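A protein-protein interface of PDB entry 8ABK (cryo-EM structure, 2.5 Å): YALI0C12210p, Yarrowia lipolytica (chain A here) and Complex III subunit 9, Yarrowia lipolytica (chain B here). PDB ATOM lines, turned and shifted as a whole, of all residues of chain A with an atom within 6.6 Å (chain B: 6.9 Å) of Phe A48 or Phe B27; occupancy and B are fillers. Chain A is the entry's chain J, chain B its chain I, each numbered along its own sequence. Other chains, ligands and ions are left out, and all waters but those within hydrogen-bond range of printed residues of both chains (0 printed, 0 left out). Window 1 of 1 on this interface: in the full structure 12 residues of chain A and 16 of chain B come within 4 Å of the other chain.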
ATOM      1  N   GLY A  43      23.653  16.171 -14.377  1.00  0.00           N
ATOM      2  CA  GLY A  43      23.887  16.691 -13.040  1.00  0.00           C
ATOM      3  C   GLY A  43      23.068  17.949 -12.776  1.00  0.00           C
ATOM      4  O   GLY A  43      22.334  18.009 -11.794  1.00  0.00           O
ATOM      5  N   ILE A  44      23.191  18.937 -13.672  1.00  0.00           N
ATOM      6  CA  ILE A  44      22.440  20.175 -13.547  1.00  0.00           C
ATOM      7  C   ILE A  44      20.951  19.840 -13.515  1.00  0.00           C
ATOM      8  O   ILE A  44      20.227  20.355 -12.672  1.00  0.00           O
ATOM      9  CB  ILE A  44      22.771  21.162 -14.686  1.00  0.00           C
ATOM     10  CG1 ILE A  44      24.248  21.566 -14.687  1.00  0.00           C
ATOM     11  CG2 ILE A  44      21.858  22.379 -14.642  1.00  0.00           C
ATOM     12  CD1 ILE A  44      24.760  22.062 -16.032  1.00  0.00           C
ATOM     13  N   GLY A  45      20.514  18.979 -14.439  1.00  0.00           N
ATOM     14  CA  GLY A  45      19.103  18.656 -14.553  1.00  0.00           C
ATOM     15  C   GLY A  45      18.577  17.990 -13.285  1.00  0.00           C
ATOM     16  O   GLY A  45      17.495  18.329 -12.809  1.00  0.00           O
ATOM     17  N   ALA A  46      19.356  17.038 -12.755  1.00  0.00           N
ATOM     18  CA  ALA A  46      18.930  16.260 -11.603  1.00  0.00           C
ATOM     19  C   ALA A  46      18.795  17.194 -10.409  1.00  0.00           C
ATOM     20  O   ALA A  46      17.769  17.204  -9.731  1.00  0.00           O
ATOM     21  CB  ALA A  46      19.912  15.151 -11.318  1.00  0.00           C
ATOM     22  N   LEU A  47      19.836  18.003 -10.210  1.00  0.00           N
ATOM     23  CA  LEU A  47      19.902  18.913  -9.084  1.00  0.00           C
ATOM     24  C   LEU A  47      18.749  19.906  -9.151  1.00  0.00           C
ATOM     25  O   LEU A  47      18.157  20.232  -8.129  1.00  0.00           O
ATOM     26  CB  LEU A  47      21.252  19.631  -9.111  1.00  0.00           C
ATOM     27  CG  LEU A  47      21.545  20.534  -7.917  1.00  0.00           C
ATOM     28  CD1 LEU A  47      21.548  19.742  -6.615  1.00  0.00           C
ATOM     29  CD2 LEU A  47      22.885  21.220  -8.102  1.00  0.00           C
ATOM     30  N   PHE A  48      18.469  20.394 -10.357  1.00  0.00           N
ATOM     31  CA  PHE A  48      17.372  21.308 -10.599  1.00  0.00           C
ATOM     32  C   PHE A  48      16.036  20.658 -10.250  1.00  0.00           C
ATOM     33  O   PHE A  48      15.162  21.338  -9.727  1.00  0.00           O
ATOM     34  CB  PHE A  48      17.400  21.723 -12.068  1.00  0.00           C
ATOM     35  CG  PHE A  48      16.356  22.724 -12.486  1.00  0.00           C
ATOM     36  CD1 PHE A  48      16.059  23.834 -11.700  1.00  0.00           C
ATOM     37  CD2 PHE A  48      15.701  22.575 -13.700  1.00  0.00           C
ATOM     38  CE1 PHE A  48      15.108  24.758 -12.112  1.00  0.00           C
ATOM     39  CE2 PHE A  48      14.764  23.508 -14.118  1.00  0.00           C
ATOM     40  CZ  PHE A  48      14.464  24.593 -13.319  1.00  0.00           C
ATOM     41  N   LEU A  49      15.868  19.368 -10.570  1.00  0.00           N
ATOM     42  CA  LEU A  49      14.612  18.680 -10.299  1.00  0.00           C
ATOM     43  C   LEU A  49      14.374  18.520  -8.802  1.00  0.00           C
ATOM     44  O   LEU A  49      13.230  18.401  -8.367  1.00  0.00           O
ATOM     45  CB  LEU A  49      14.613  17.304 -10.962  1.00  0.00           C
ATOM     46  CG  LEU A  49      14.074  17.271 -12.386  1.00  0.00           C
ATOM     47  CD1 LEU A  49      14.266  15.887 -12.983  1.00  0.00           C
ATOM     48  CD2 LEU A  49      12.602  17.656 -12.418  1.00  0.00           C
ATOM     49  N   ILE A  50      15.453  18.465  -8.015  1.00  0.00           N
ATOM     50  CA  ILE A  50      15.257  18.214  -6.597  1.00  0.00           C
ATOM     51  C   ILE A  50      15.622  19.450  -5.796  1.00  0.00           C
ATOM     52  O   ILE A  50      15.860  19.361  -4.596  1.00  0.00           O
ATOM     53  CB  ILE A  50      16.026  16.973  -6.115  1.00  0.00           C
ATOM     54  CG1 ILE A  50      17.531  17.123  -6.356  1.00  0.00           C
ATOM     55  CG2 ILE A  50      15.425  15.709  -6.720  1.00  0.00           C
ATOM     56  CD1 ILE A  50      18.385  16.192  -5.538  1.00  0.00           C
ATOM     57  N   GLU A  51      15.632  20.598  -6.467  1.00  0.00           N
ATOM     58  CA  GLU A  51      15.963  21.848  -5.815  1.00  0.00           C
ATOM     59  C   GLU A  51      14.954  22.143  -4.705  1.00  0.00           C
ATOM     60  O   GLU A  51      15.283  22.785  -3.712  1.00  0.00           O
ATOM     61  CB  GLU A  51      15.997  22.946  -6.875  1.00  0.00           C
ATOM     62  CG  GLU A  51      16.172  24.352  -6.317  1.00  0.00           C
ATOM     63  CD  GLU A  51      14.936  25.082  -5.803  1.00  0.00           C
ATOM     64  OE1 GLU A  51      13.834  24.843  -6.350  1.00  0.00           O
ATOM     65  OE2 GLU A  51      15.075  25.921  -4.870  1.00  0.00           O
ATOM     66  N   GLY A  52      13.713  21.700  -4.898  1.00  0.00           N
ATOM     67  CA  GLY A  52      12.669  21.946  -3.919  1.00  0.00           C
ATOM     68  C   GLY A  52      12.794  21.050  -2.686  1.00  0.00           C
ATOM     69  O   GLY A  52      12.381  21.436  -1.597  1.00  0.00           O
ATOM     70  N   LEU A  61      22.659  23.211  -1.668  1.00  0.00           N
ATOM     71  CA  LEU A  61      22.501  24.490  -2.341  1.00  0.00           C
ATOM     72  C   LEU A  61      22.848  25.659  -1.421  1.00  0.00           C
ATOM     73  O   LEU A  61      23.303  26.686  -1.898  1.00  0.00           O
ATOM     74  CB  LEU A  61      21.072  24.616  -2.871  1.00  0.00           C
ATOM     75  CG  LEU A  61      20.700  23.654  -3.998  1.00  0.00           C
ATOM     76  CD1 LEU A  61      19.219  23.763  -4.374  1.00  0.00           C
ATOM     77  CD2 LEU A  61      21.601  23.853  -5.212  1.00  0.00           C
ATOM     78  N   TRP A  71      18.795  30.092  -0.436  1.00  0.00           N
ATOM     79  CA  TRP A  71      18.096  28.910   0.036  1.00  0.00           C
ATOM     80  C   TRP A  71      18.044  28.861   1.559  1.00  0.00           C
ATOM     81  O   TRP A  71      17.571  27.873   2.121  1.00  0.00           O
ATOM     82  CB  TRP A  71      18.726  27.646  -0.556  1.00  0.00           C
ATOM     83  CG  TRP A  71      18.490  27.505  -2.027  1.00  0.00           C
ATOM     84  CD1 TRP A  71      17.361  27.050  -2.645  1.00  0.00           C
ATOM     85  CD2 TRP A  71      19.412  27.833  -3.076  1.00  0.00           C
ATOM     86  NE1 TRP A  71      17.517  27.067  -4.004  1.00  0.00           N
ATOM     87  CE2 TRP A  71      18.763  27.545  -4.299  1.00  0.00           C
ATOM     88  CE3 TRP A  71      20.723  28.328  -3.096  1.00  0.00           C
ATOM     89  CZ2 TRP A  71      19.390  27.730  -5.531  1.00  0.00           C
ATOM     90  CZ3 TRP A  71      21.339  28.519  -4.314  1.00  0.00           C
ATOM     91  CH2 TRP A  71      20.677  28.222  -5.511  1.00  0.00           C
ATOM     92  N   ILE B  22      20.888  25.147 -21.686  1.00  0.00           N
ATOM     93  CA  ILE B  22      19.459  25.374 -21.535  1.00  0.00           C
ATOM     94  C   ILE B  22      19.048  25.044 -20.101  1.00  0.00           C
ATOM     95  O   ILE B  22      18.346  25.840 -19.489  1.00  0.00           O
ATOM     96  CB  ILE B  22      18.658  24.583 -22.594  1.00  0.00           C
ATOM     97  CG1 ILE B  22      18.830  25.199 -23.987  1.00  0.00           C
ATOM     98  CG2 ILE B  22      17.186  24.449 -22.208  1.00  0.00           C
ATOM     99  CD1 ILE B  22      18.451  24.270 -25.127  1.00  0.00           C
ATOM    100  N   LEU B  23      19.514  23.899 -19.567  1.00  0.00           N
ATOM    101  CA  LEU B  23      19.166  23.477 -18.217  1.00  0.00           C
ATOM    102  C   LEU B  23      19.729  24.436 -17.178  1.00  0.00           C
ATOM    103  O   LEU B  23      19.030  24.766 -16.229  1.00  0.00           O
ATOM    104  CB  LEU B  23      19.599  22.033 -17.947  1.00  0.00           C
ATOM    105  CG  LEU B  23      18.872  20.987 -18.794  1.00  0.00           C
ATOM    106  CD1 LEU B  23      19.337  19.584 -18.471  1.00  0.00           C
ATOM    107  CD2 LEU B  23      17.353  21.096 -18.683  1.00  0.00           C
ATOM    108  N   ALA B  24      20.969  24.895 -17.370  1.00  0.00           N
ATOM    109  CA  ALA B  24      21.557  25.818 -16.412  1.00  0.00           C
ATOM    110  C   ALA B  24      20.815  27.155 -16.435  1.00  0.00           C
ATOM    111  O   ALA B  24      20.585  27.747 -15.385  1.00  0.00           O
ATOM    112  CB  ALA B  24      23.032  25.976 -16.673  1.00  0.00           C
ATOM    113  N   SER B  25      20.412  27.603 -17.629  1.00  0.00           N
ATOM    114  CA  SER B  25      19.613  28.812 -17.767  1.00  0.00           C
ATOM    115  C   SER B  25      18.248  28.639 -17.113  1.00  0.00           C
ATOM    116  O   SER B  25      17.719  29.597 -16.561  1.00  0.00           O
ATOM    117  CB  SER B  25      19.435  29.176 -19.206  1.00  0.00           C
ATOM    118  OG  SER B  25      20.689  29.233 -19.850  1.00  0.00           O
ATOM    119  N   ALA B  26      17.663  27.439 -17.230  1.00  0.00           N
ATOM    120  CA  ALA B  26      16.356  27.190 -16.641  1.00  0.00           C
ATOM    121  C   ALA B  26      16.463  27.274 -15.122  1.00  0.00           C
ATOM    122  O   ALA B  26      15.569  27.825 -14.493  1.00  0.00           O
ATOM    123  CB  ALA B  26      15.764  25.882 -17.111  1.00  0.00           C
ATOM    124  N   PHE B  27      17.576  26.770 -14.565  1.00  0.00           N
ATOM    125  CA  PHE B  27      17.842  26.841 -13.136  1.00  0.00           C
ATOM    126  C   PHE B  27      17.935  28.304 -12.700  1.00  0.00           C
ATOM    127  O   PHE B  27      17.247  28.709 -11.762  1.00  0.00           O
ATOM    128  CB  PHE B  27      19.100  26.043 -12.795  1.00  0.00           C
ATOM    129  CG  PHE B  27      19.180  25.455 -11.411  1.00  0.00           C
ATOM    130  CD1 PHE B  27      18.701  26.134 -10.298  1.00  0.00           C
ATOM    131  CD2 PHE B  27      19.793  24.225 -11.212  1.00  0.00           C
ATOM    132  CE1 PHE B  27      18.802  25.587  -9.025  1.00  0.00           C
ATOM    133  CE2 PHE B  27      19.901  23.678  -9.940  1.00  0.00           C
ATOM    134  CZ  PHE B  27      19.404  24.359  -8.848  1.00  0.00           C
ATOM    135  N   VAL B  28      18.717  29.103 -13.431  1.00  0.00           N
ATOM    136  CA  VAL B  28      18.885  30.510 -13.104  1.00  0.00           C
ATOM    137  C   VAL B  28      17.559  31.247 -13.234  1.00  0.00           C
ATOM    138  O   VAL B  28      17.188  31.967 -12.315  1.00  0.00           O
ATOM    139  CB  VAL B  28      20.000  31.182 -13.926  1.00  0.00           C
ATOM    140  CG1 VAL B  28      20.036  32.687 -13.707  1.00  0.00           C
ATOM    141  CG2 VAL B  28      21.348  30.573 -13.592  1.00  0.00           C
ATOM    142  N   PHE B  29      16.853  31.035 -14.346  1.00  0.00           N
ATOM    143  CA  PHE B  29      15.577  31.691 -14.572  1.00  0.00           C
ATOM    144  C   PHE B  29      14.618  31.388 -13.425  1.00  0.00           C
ATOM    145  O   PHE B  29      14.076  32.309 -12.827  1.00  0.00           O
ATOM    146  CB  PHE B  29      14.960  31.262 -15.899  1.00  0.00           C
ATOM    147  CG  PHE B  29      13.530  31.709 -16.049  1.00  0.00           C
ATOM    148  CD1 PHE B  29      13.232  32.988 -16.503  1.00  0.00           C
ATOM    149  CD2 PHE B  29      12.478  30.864 -15.709  1.00  0.00           C
ATOM    150  CE1 PHE B  29      11.915  33.412 -16.625  1.00  0.00           C
ATOM    151  CE2 PHE B  29      11.158  31.287 -15.832  1.00  0.00           C
ATOM    152  CZ  PHE B  29      10.879  32.562 -16.282  1.00  0.00           C
ATOM    153  N   ASP B  30      14.463  30.103 -13.092  1.00  0.00           N
ATOM    154  CA  ASP B  30      13.583  29.642 -12.030  1.00  0.00           C
ATOM    155  C   ASP B  30      13.849  30.378 -10.715  1.00  0.00           C
ATOM    156  O   ASP B  30      12.901  30.804 -10.069  1.00  0.00           O
ATOM    157  CB  ASP B  30      13.722  28.136 -11.828  1.00  0.00           C
ATOM    158  CG  ASP B  30      12.497  27.494 -11.201  1.00  0.00           C
ATOM    159  OD1 ASP B  30      11.465  27.380 -11.905  1.00  0.00           O
ATOM    160  OD2 ASP B  30      12.573  27.110 -10.018  1.00  0.00           O
ATOM    161  N   MET B  31      15.119  30.527 -10.321  1.00  0.00           N
ATOM    162  CA  MET B  31      15.473  31.169  -9.063  1.00  0.00           C
ATOM    163  C   MET B  31      15.253  32.681  -9.101  1.00  0.00           C
ATOM    164  O   MET B  31      14.775  33.274  -8.135  1.00  0.00           O
ATOM    165  CB  MET B  31      16.930  30.883  -8.694  1.00  0.00           C
ATOM    166  CG  MET B  31      17.217  29.397  -8.563  1.00  0.00           C
ATOM    167  SD  MET B  31      16.315  28.471  -7.280  1.00  0.00           S
ATOM    168  CE  MET B  31      14.923  27.791  -8.188  1.00  0.00           C
ATOM    169  N   THR B  32      15.577  33.307 -10.227  1.00  0.00           N
ATOM    170  CA  THR B  32      15.495  34.752 -10.320  1.00  0.00           C
ATOM    171  C   THR B  32      14.047  35.178 -10.505  1.00  0.00           C
ATOM    172  O   THR B  32      13.637  36.160  -9.914  1.00  0.00           O
ATOM    173  CB  THR B  32      16.441  35.286 -11.396  1.00  0.00           C
ATOM    174  OG1 THR B  32      16.094  34.535 -12.556  1.00  0.00           O
ATOM    175  CG2 THR B  32      17.881  34.991 -11.052  1.00  0.00           C
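The side-chain carboxylate (OE2) of Glu A51 sits at hydrogen-bond distance from the indole nitrogen (NE1) of Trp A71, at 2.8 Å.
Among the printed residues, merely in contact across the chains: Ile A44 with Leu B23 (3.9 Å), Ile A44 with Ala B24 (3.8 Å), Phe A48 with Ala B26 (3.6 Å), Phe A48 with Phe B27 (3.5 Å), Phe A48 with Asp B30 (3.7 Å) and Glu A51 with Phe B27 (3.97 Å).
OE2 of Glu A51 lies close to SD of Met B31, at 3.7 Å. The indole nitrogen (NE1) of Trp A71 lies close to the side-chain sulfur (SD) of Met B31, at 3.8 Å.
Hydrophobic or aromatic side chains of chain A that line the printed part of chain B: Ile A44, Phe A48 and Trp A71. Of the 11 printed residues of chain B, 6 touch a printed residue of chain A. Printed residues of chain B that touch a printed residue of chain A: Leu B23, Ala B24, Ala B26, Phe B27, Asp B30 and Met B31. Among the printed residues, 8 pairs touch across the chains.
Phe A48 touches just these residues of chain B: Ala B26, Phe B27 and Asp B30. Of the printed residues of chain A, Ala B26 touches Phe A48 (3.6 Å). Printed residues of chain A within 4 Å of Ala B24: Ile A44.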
